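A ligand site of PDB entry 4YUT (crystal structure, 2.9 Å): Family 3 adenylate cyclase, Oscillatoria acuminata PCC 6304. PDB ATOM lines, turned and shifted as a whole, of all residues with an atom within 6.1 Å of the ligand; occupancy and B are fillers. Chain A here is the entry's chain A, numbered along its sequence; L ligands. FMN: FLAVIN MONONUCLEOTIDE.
OD2 of Asp 83 sits at hydrogen-bond distance from O2' of the ligand (2.8 Å).
The guanidinium group of Arg 79 lies within hydrogen-bond range of an oxygen (O4') of the ligand (2.8 Å).
The side-chain amide oxygen (OD1) of Asn 46 lies close to an oxygen (O4) of the ligand, 3.5 Å away.
NE2 of Gln 64 sits at hydrogen-bond distance from N5 of the ligand, 3.1 Å away.
A ring nitrogen (ND1) of His 86 is in hydrogen-bond range of the backbone carbonyl oxygen (O) of Ile 80 (3.3 Å).
The side-chain amide nitrogen (ND2) of Asn 46 is in hydrogen-bond range of the side-chain sulfur (SD) of Met 108, 3.2 Å away.
The backbone NH of Phe 62 lies within hydrogen-bond range of the backbone carbonyl oxygen of Ser 24 (2.8 Å).
The side-chain carboxylate (OD1) of Asp 83 is in salt-bridge range of the guanidinium group (NE) of Arg 85 (2.8 Å).
A ring nitrogen (NE2) of His 86 lies close to the side-chain hydroxyl of Ser 24 (3.3 Å).
O of Asn 46 sits at hydrogen-bond distance from N of Val 51, at 3.3 Å.
OG of Ser 42 lies within hydrogen-bond range of O of Ile 38, 2.7 Å away.
The side-chain amide oxygen (OE1) of Gln 64 is in hydrogen-bond range of the side-chain hydroxyl (OH) of Tyr 22 (2.7 Å).
SD of Met 108 lies close to O4 of the ligand (3.2 Å).
Tyr 22 touches the ligand.
Ile 38 touches the ligand.
CB of Ser 42 touches C4A of the ligand, 3.6 Å away.
CE of Lys 45 touches O1P of the ligand, at 3.3 Å.
Leu 55 touches the ligand.
Phe 62 touches the ligand.
Leu 66 touches the ligand (CD2 to O4, 3.3 Å).
CG2 of Ile 76 touches N3 of the ligand, 3.3 Å away.
CD1 of Ile 80 touches C4A of the ligand, at 3.6 Å.
NE2 of His 86 touches C7M of the ligand, 3.2 Å away.
Hydrophobic or aromatic side chains that line the ligand: Ile 38, Leu 55, Phe 62, Leu 66, Ile 76, Ile 80, His 86 and Met 108.
Within 4 Å of the ligand: Tyr 22, Ile 38, Ser 42, Lys 45, Asn 46, Leu 55, Phe 62, Gln 64, Leu 66, Ile 76, Arg 79, Ile 80, Asp 83, His 86 and Met 108.
The nearest printed residue that does not touch the ligand is Ile 41 (4.002 Å).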
ATOM      1  N   TYR A  22       7.081  10.401   2.378  1.00  0.00           N
ATOM      2  CA  TYR A  22       7.987   9.349   2.850  1.00  0.00           C
ATOM      3  C   TYR A  22       8.903   8.765   1.781  1.00  0.00           C
ATOM      4  O   TYR A  22       8.571   8.776   0.593  1.00  0.00           O
ATOM      5  CB  TYR A  22       7.214   8.213   3.572  1.00  0.00           C
ATOM      6  CG  TYR A  22       6.459   7.260   2.673  1.00  0.00           C
ATOM      7  CD1 TYR A  22       5.070   7.298   2.594  1.00  0.00           C
ATOM      8  CD2 TYR A  22       7.121   6.244   1.978  1.00  0.00           C
ATOM      9  CE1 TYR A  22       4.366   6.393   1.791  1.00  0.00           C
ATOM     10  CE2 TYR A  22       6.433   5.357   1.151  1.00  0.00           C
ATOM     11  CZ  TYR A  22       5.054   5.438   1.061  1.00  0.00           C
ATOM     12  OH  TYR A  22       4.381   4.577   0.237  1.00  0.00           O
ATOM     13  N   SER A  24      10.740   5.140   0.788  1.00  0.00           N
ATOM     14  CA  SER A  24      10.728   3.692   0.919  1.00  0.00           C
ATOM     15  C   SER A  24      11.775   3.070  -0.032  1.00  0.00           C
ATOM     16  O   SER A  24      12.203   3.730  -0.983  1.00  0.00           O
ATOM     17  CB  SER A  24       9.322   3.174   0.605  1.00  0.00           C
ATOM     18  OG  SER A  24       9.310   1.802   0.218  1.00  0.00           O
ATOM     19  N   ILE A  38       0.736  -1.314  -8.511  1.00  0.00           N
ATOM     20  CA  ILE A  38       0.871  -0.479  -7.305  1.00  0.00           C
ATOM     21  C   ILE A  38       0.087   0.823  -7.486  1.00  0.00           C
ATOM     22  O   ILE A  38      -0.624   1.236  -6.575  1.00  0.00           O
ATOM     23  CB  ILE A  38       2.372  -0.234  -6.964  1.00  0.00           C
ATOM     24  CG1 ILE A  38       3.119  -1.558  -6.718  1.00  0.00           C
ATOM     25  CG2 ILE A  38       2.520   0.712  -5.770  1.00  0.00           C
ATOM     26  CD1 ILE A  38       4.620  -1.526  -7.011  1.00  0.00           C
ATOM     27  N   ILE A  41      -4.091  -0.132  -8.094  1.00  0.00           N
ATOM     28  CA  ILE A  41      -4.774  -0.514  -6.858  1.00  0.00           C
ATOM     29  C   ILE A  41      -4.932   0.689  -5.905  1.00  0.00           C
ATOM     30  O   ILE A  41      -5.998   0.853  -5.290  1.00  0.00           O
ATOM     31  CB  ILE A  41      -4.092  -1.755  -6.187  1.00  0.00           C
ATOM     32  CG1 ILE A  41      -4.078  -2.976  -7.149  1.00  0.00           C
ATOM     33  CG2 ILE A  41      -4.750  -2.120  -4.854  1.00  0.00           C
ATOM     34  CD1 ILE A  41      -2.904  -3.997  -6.950  1.00  0.00           C
ATOM     35  N   SER A  42      -3.884   1.522  -5.792  1.00  0.00           N
ATOM     36  CA  SER A  42      -3.829   2.703  -4.922  1.00  0.00           C
ATOM     37  C   SER A  42      -4.816   3.803  -5.303  1.00  0.00           C
ATOM     38  O   SER A  42      -5.590   4.251  -4.450  1.00  0.00           O
ATOM     39  CB  SER A  42      -2.405   3.257  -4.847  1.00  0.00           C
ATOM     40  OG  SER A  42      -1.932   3.575  -6.140  1.00  0.00           O
ATOM     41  N   SER A  43      -4.792   4.248  -6.578  1.00  0.00           N
ATOM     42  CA  SER A  43      -5.648   5.303  -7.107  1.00  0.00           C
ATOM     43  C   SER A  43      -7.150   5.063  -6.911  1.00  0.00           C
ATOM     44  O   SER A  43      -7.875   6.005  -6.580  1.00  0.00           O
ATOM     45  CB  SER A  43      -5.321   5.581  -8.574  1.00  0.00           C
ATOM     46  OG  SER A  43      -5.160   4.381  -9.319  1.00  0.00           O
ATOM     47  N   LYS A  45      -8.515   2.940  -4.580  1.00  0.00           N
ATOM     48  CA  LYS A  45      -8.740   2.931  -3.124  1.00  0.00           C
ATOM     49  C   LYS A  45      -8.787   4.379  -2.606  1.00  0.00           C
ATOM     50  O   LYS A  45      -9.582   4.680  -1.713  1.00  0.00           O
ATOM     51  CB  LYS A  45      -7.629   2.132  -2.414  1.00  0.00           C
ATOM     52  CG  LYS A  45      -7.843   0.626  -2.431  1.00  0.00           C
ATOM     53  CD  LYS A  45      -7.985   0.068  -1.023  1.00  0.00           C
ATOM     54  CE  LYS A  45      -8.365  -1.401  -1.005  1.00  0.00           C
ATOM     55  NZ  LYS A  45      -9.824  -1.613  -1.174  1.00  0.00           N
ATOM     56  N   ASN A  46      -7.946   5.255  -3.210  1.00  0.00           N
ATOM     57  CA  ASN A  46      -7.840   6.692  -2.926  1.00  0.00           C
ATOM     58  C   ASN A  46      -9.155   7.407  -3.186  1.00  0.00           C
ATOM     59  O   ASN A  46      -9.537   8.249  -2.386  1.00  0.00           O
ATOM     60  CB  ASN A  46      -6.746   7.316  -3.814  1.00  0.00           C
ATOM     61  CG  ASN A  46      -5.379   7.493  -3.189  1.00  0.00           C
ATOM     62  OD1 ASN A  46      -4.901   6.662  -2.390  1.00  0.00           O
ATOM     63  ND2 ASN A  46      -4.705   8.558  -3.586  1.00  0.00           N
ATOM     64  N   VAL A  51      -9.038  10.749  -0.300  1.00  0.00           N
ATOM     65  CA  VAL A  51      -7.645  11.177  -0.209  1.00  0.00           C
ATOM     66  C   VAL A  51      -6.936  11.224  -1.589  1.00  0.00           C
ATOM     67  O   VAL A  51      -7.315  10.507  -2.524  1.00  0.00           O
ATOM     68  CB  VAL A  51      -6.818  10.347   0.837  1.00  0.00           C
ATOM     69  CG1 VAL A  51      -7.624  10.069   2.103  1.00  0.00           C
ATOM     70  CG2 VAL A  51      -6.231   9.067   0.245  1.00  0.00           C
ATOM     71  N   LEU A  55       2.893   9.254  -6.285  1.00  0.00           N
ATOM     72  CA  LEU A  55       3.838   8.166  -6.053  1.00  0.00           C
ATOM     73  C   LEU A  55       4.939   8.271  -7.120  1.00  0.00           C
ATOM     74  O   LEU A  55       4.649   8.659  -8.238  1.00  0.00           O
ATOM     75  CB  LEU A  55       3.106   6.803  -6.105  1.00  0.00           C
ATOM     76  CG  LEU A  55       3.820   5.499  -5.619  1.00  0.00           C
ATOM     77  CD1 LEU A  55       4.506   4.759  -6.767  1.00  0.00           C
ATOM     78  CD2 LEU A  55       4.770   5.740  -4.444  1.00  0.00           C
ATOM     79  N   PHE A  62      11.337   4.662  -3.511  1.00  0.00           N
ATOM     80  CA  PHE A  62       9.976   5.170  -3.696  1.00  0.00           C
ATOM     81  C   PHE A  62       9.907   6.522  -3.007  1.00  0.00           C
ATOM     82  O   PHE A  62      10.725   6.805  -2.129  1.00  0.00           O
ATOM     83  CB  PHE A  62       8.930   4.224  -3.062  1.00  0.00           C
ATOM     84  CG  PHE A  62       8.470   3.016  -3.844  1.00  0.00           C
ATOM     85  CD1 PHE A  62       7.762   3.160  -5.032  1.00  0.00           C
ATOM     86  CD2 PHE A  62       8.659   1.732  -3.337  1.00  0.00           C
ATOM     87  CE1 PHE A  62       7.302   2.034  -5.731  1.00  0.00           C
ATOM     88  CE2 PHE A  62       8.188   0.613  -4.037  1.00  0.00           C
ATOM     89  CZ  PHE A  62       7.513   0.772  -5.226  1.00  0.00           C
ATOM     90  N   GLN A  64       6.536   9.271  -1.772  1.00  0.00           N
ATOM     91  CA  GLN A  64       5.083   9.358  -1.837  1.00  0.00           C
ATOM     92  C   GLN A  64       4.466  10.439  -0.967  1.00  0.00           C
ATOM     93  O   GLN A  64       4.630  10.419   0.246  1.00  0.00           O
ATOM     94  CB  GLN A  64       4.423   7.991  -1.519  1.00  0.00           C
ATOM     95  CG  GLN A  64       2.888   8.005  -1.479  1.00  0.00           C
ATOM     96  CD  GLN A  64       2.281   6.626  -1.541  1.00  0.00           C
ATOM     97  OE1 GLN A  64       2.153   5.920  -0.547  1.00  0.00           O
ATOM     98  NE2 GLN A  64       1.862   6.217  -2.716  1.00  0.00           N
ATOM     99  N   LEU A  66       0.807  11.923   0.440  1.00  0.00           N
ATOM    100  CA  LEU A  66      -0.552  11.430   0.722  1.00  0.00           C
ATOM    101  C   LEU A  66      -1.299  12.468   1.534  1.00  0.00           C
ATOM    102  O   LEU A  66      -0.850  12.826   2.611  1.00  0.00           O
ATOM    103  CB  LEU A  66      -0.503  10.088   1.470  1.00  0.00           C
ATOM    104  CG  LEU A  66      -0.361   8.835   0.605  1.00  0.00           C
ATOM    105  CD1 LEU A  66       0.315   7.712   1.381  1.00  0.00           C
ATOM    106  CD2 LEU A  66      -1.717   8.394   0.052  1.00  0.00           C
ATOM    107  N   ILE A  76      -4.622   4.132   5.783  1.00  0.00           N
ATOM    108  CA  ILE A  76      -4.028   3.860   4.475  1.00  0.00           C
ATOM    109  C   ILE A  76      -2.516   3.630   4.633  1.00  0.00           C
ATOM    110  O   ILE A  76      -2.008   2.631   4.138  1.00  0.00           O
ATOM    111  CB  ILE A  76      -4.386   4.941   3.407  1.00  0.00           C
ATOM    112  CG1 ILE A  76      -5.907   5.092   3.264  1.00  0.00           C
ATOM    113  CG2 ILE A  76      -3.771   4.596   2.034  1.00  0.00           C
ATOM    114  CD1 ILE A  76      -6.385   6.480   2.919  1.00  0.00           C
ATOM    115  N   ARG A  79      -1.517   0.101   6.104  1.00  0.00           N
ATOM    116  CA  ARG A  79      -1.424  -0.974   5.105  1.00  0.00           C
ATOM    117  C   ARG A  79      -0.113  -0.814   4.324  1.00  0.00           C
ATOM    118  O   ARG A  79       0.532  -1.828   4.006  1.00  0.00           O
ATOM    119  CB  ARG A  79      -2.616  -0.947   4.138  1.00  0.00           C
ATOM    120  CG  ARG A  79      -3.996  -0.942   4.803  1.00  0.00           C
ATOM    121  CD  ARG A  79      -5.091  -1.425   3.866  1.00  0.00           C
ATOM    122  NE  ARG A  79      -5.431  -0.475   2.808  1.00  0.00           N
ATOM    123  CZ  ARG A  79      -6.357   0.480   2.922  1.00  0.00           C
ATOM    124  NH1 ARG A  79      -6.608   1.300   1.906  1.00  0.00           N
ATOM    125  NH2 ARG A  79      -7.039   0.631   4.052  1.00  0.00           N
ATOM    126  N   ILE A  80       0.287   0.436   4.033  1.00  0.00           N
ATOM    127  CA  ILE A  80       1.517   0.768   3.292  1.00  0.00           C
ATOM    128  C   ILE A  80       2.776   0.379   4.127  1.00  0.00           C
ATOM    129  O   ILE A  80       3.817   0.010   3.562  1.00  0.00           O
ATOM    130  CB  ILE A  80       1.517   2.252   2.810  1.00  0.00           C
ATOM    131  CG1 ILE A  80       0.308   2.543   1.877  1.00  0.00           C
ATOM    132  CG2 ILE A  80       2.823   2.605   2.096  1.00  0.00           C
ATOM    133  CD1 ILE A  80      -0.100   4.001   1.811  1.00  0.00           C
ATOM    134  N   LEU A  81       2.635   0.418   5.476  1.00  0.00           N
ATOM    135  CA  LEU A  81       3.661   0.043   6.441  1.00  0.00           C
ATOM    136  C   LEU A  81       3.801  -1.492   6.533  1.00  0.00           C
ATOM    137  O   LEU A  81       4.760  -1.993   7.123  1.00  0.00           O
ATOM    138  CB  LEU A  81       3.345   0.617   7.836  1.00  0.00           C
ATOM    139  CG  LEU A  81       3.644   2.097   8.073  1.00  0.00           C
ATOM    140  CD1 LEU A  81       3.114   2.535   9.428  1.00  0.00           C
ATOM    141  CD2 LEU A  81       5.137   2.404   7.943  1.00  0.00           C
ATOM    142  N   ALA A  82       2.822  -2.230   5.971  1.00  0.00           N
ATOM    143  CA  ALA A  82       2.780  -3.687   5.961  1.00  0.00           C
ATOM    144  C   ALA A  82       2.983  -4.322   4.566  1.00  0.00           C
ATOM    145  O   ALA A  82       2.979  -5.543   4.476  1.00  0.00           O
ATOM    146  CB  ALA A  82       1.498  -4.175   6.613  1.00  0.00           C
ATOM    147  N   ASP A  83       3.190  -3.513   3.512  1.00  0.00           N
ATOM    148  CA  ASP A  83       3.420  -4.067   2.169  1.00  0.00           C
ATOM    149  C   ASP A  83       4.855  -4.621   2.047  1.00  0.00           C
ATOM    150  O   ASP A  83       5.802  -3.973   2.477  1.00  0.00           O
ATOM    151  CB  ASP A  83       3.128  -3.033   1.073  1.00  0.00           C
ATOM    152  CG  ASP A  83       2.983  -3.622  -0.322  1.00  0.00           C
ATOM    153  OD1 ASP A  83       3.956  -4.233  -0.804  1.00  0.00           O
ATOM    154  OD2 ASP A  83       1.900  -3.444  -0.927  1.00  0.00           O
ATOM    155  N   ARG A  85       6.812  -5.024  -0.595  1.00  0.00           N
ATOM    156  CA  ARG A  85       7.638  -4.263  -1.551  1.00  0.00           C
ATOM    157  C   ARG A  85       8.502  -3.152  -0.885  1.00  0.00           C
ATOM    158  O   ARG A  85       9.329  -2.527  -1.563  1.00  0.00           O
ATOM    159  CB  ARG A  85       6.723  -3.634  -2.622  1.00  0.00           C
ATOM    160  CG  ARG A  85       6.353  -4.544  -3.796  1.00  0.00           C
ATOM    161  CD  ARG A  85       5.083  -5.357  -3.626  1.00  0.00           C
ATOM    162  NE  ARG A  85       3.868  -4.552  -3.550  1.00  0.00           N
ATOM    163  CZ  ARG A  85       2.627  -5.035  -3.729  1.00  0.00           C
ATOM    164  NH1 ARG A  85       1.577  -4.241  -3.621  1.00  0.00           N
ATOM    165  NH2 ARG A  85       2.454  -6.312  -4.028  1.00  0.00           N
ATOM    166  N   HIS A  86       8.343  -2.958   0.441  1.00  0.00           N
ATOM    167  CA  HIS A  86       8.941  -1.909   1.257  1.00  0.00           C
ATOM    168  C   HIS A  86      10.033  -2.324   2.237  1.00  0.00           C
ATOM    169  O   HIS A  86      10.042  -3.441   2.741  1.00  0.00           O
ATOM    170  CB  HIS A  86       7.815  -1.229   2.056  1.00  0.00           C
ATOM    171  CG  HIS A  86       7.084  -0.179   1.288  1.00  0.00           C
ATOM    172  ND1 HIS A  86       6.566   0.923   1.924  1.00  0.00           N
ATOM    173  CD2 HIS A  86       6.822  -0.096  -0.036  1.00  0.00           C
ATOM    174  CE1 HIS A  86       6.006   1.661   0.971  1.00  0.00           C
ATOM    175  NE2 HIS A  86       6.145   1.082  -0.223  1.00  0.00           N
ATOM    176  N   MET A 108      -3.390   9.774  -6.670  1.00  0.00           N
ATOM    177  CA  MET A 108      -2.272   8.838  -6.819  1.00  0.00           C
ATOM    178  C   MET A 108      -1.738   8.716  -8.256  1.00  0.00           C
ATOM    179  O   MET A 108      -1.686   7.615  -8.826  1.00  0.00           O
ATOM    180  CB  MET A 108      -2.606   7.456  -6.224  1.00  0.00           C
ATOM    181  CG  MET A 108      -1.575   6.971  -5.243  1.00  0.00           C
ATOM    182  SD  MET A 108      -1.602   7.927  -3.710  1.00  0.00           S
ATOM    183  CE  MET A 108      -0.017   8.550  -3.729  1.00  0.00           C
HETATM  184  N1  FMN L   1      -2.566   1.555  -1.121  1.00  0.00           N
HETATM  185  C2  FMN L   1      -3.502   2.544  -0.956  1.00  0.00           C
HETATM  186  O2  FMN L   1      -4.651   2.300  -0.585  1.00  0.00           O
HETATM  187  N3  FMN L   1      -3.146   3.876  -1.150  1.00  0.00           N
HETATM  188  C4  FMN L   1      -1.888   4.331  -1.478  1.00  0.00           C
HETATM  189  O4  FMN L   1      -1.697   5.536  -1.646  1.00  0.00           O
HETATM  190  C4A FMN L   1      -0.876   3.281  -1.620  1.00  0.00           C
HETATM  191  N5  FMN L   1       0.356   3.624  -1.887  1.00  0.00           N
HETATM  192  C5A FMN L   1       1.307   2.618  -1.993  1.00  0.00           C
HETATM  193  C6  FMN L   1       2.618   2.970  -2.319  1.00  0.00           C
HETATM  194  C7  FMN L   1       3.597   2.006  -2.512  1.00  0.00           C
HETATM  195  C7M FMN L   1       4.991   2.437  -2.914  1.00  0.00           C
HETATM  196  C8  FMN L   1       3.271   0.636  -2.345  1.00  0.00           C
HETATM  197  C8M FMN L   1       4.279  -0.454  -2.597  1.00  0.00           C
HETATM  198  C9  FMN L   1       1.968   0.301  -2.002  1.00  0.00           C
HETATM  199  C9A FMN L   1       0.981   1.261  -1.833  1.00  0.00           C
HETATM  200  N10 FMN L   1      -0.366   0.937  -1.546  1.00  0.00           N
HETATM  201  C10 FMN L   1      -1.318   1.906  -1.421  1.00  0.00           C
HETATM  202  C1' FMN L   1      -0.731  -0.494  -1.453  1.00  0.00           C
HETATM  203  C2' FMN L   1      -0.785  -1.026  -0.023  1.00  0.00           C
HETATM  204  O2' FMN L   1       0.522  -1.442   0.402  1.00  0.00           O
HETATM  205  C3' FMN L   1      -1.748  -2.204   0.095  1.00  0.00           C
HETATM  206  O3' FMN L   1      -1.475  -3.158  -0.942  1.00  0.00           O
HETATM  207  C4' FMN L   1      -3.226  -1.808   0.029  1.00  0.00           C
HETATM  208  O4' FMN L   1      -3.483  -0.668   0.857  1.00  0.00           O
HETATM  209  C5' FMN L   1      -4.158  -2.946   0.383  1.00  0.00           C
HETATM  210  O5' FMN L   1      -4.850  -3.303  -0.824  1.00  0.00           O
HETATM  211  P   FMN L   1      -6.019  -4.394  -0.776  1.00  0.00           P
HETATM  212  O1P FMN L   1      -6.958  -4.103   0.373  1.00  0.00           O
HETATM  213  O2P FMN L   1      -6.703  -4.342  -2.159  1.00  0.00           O
HETATM  214  O3P FMN L   1      -5.287  -5.738  -0.648  1.00  0.00           O
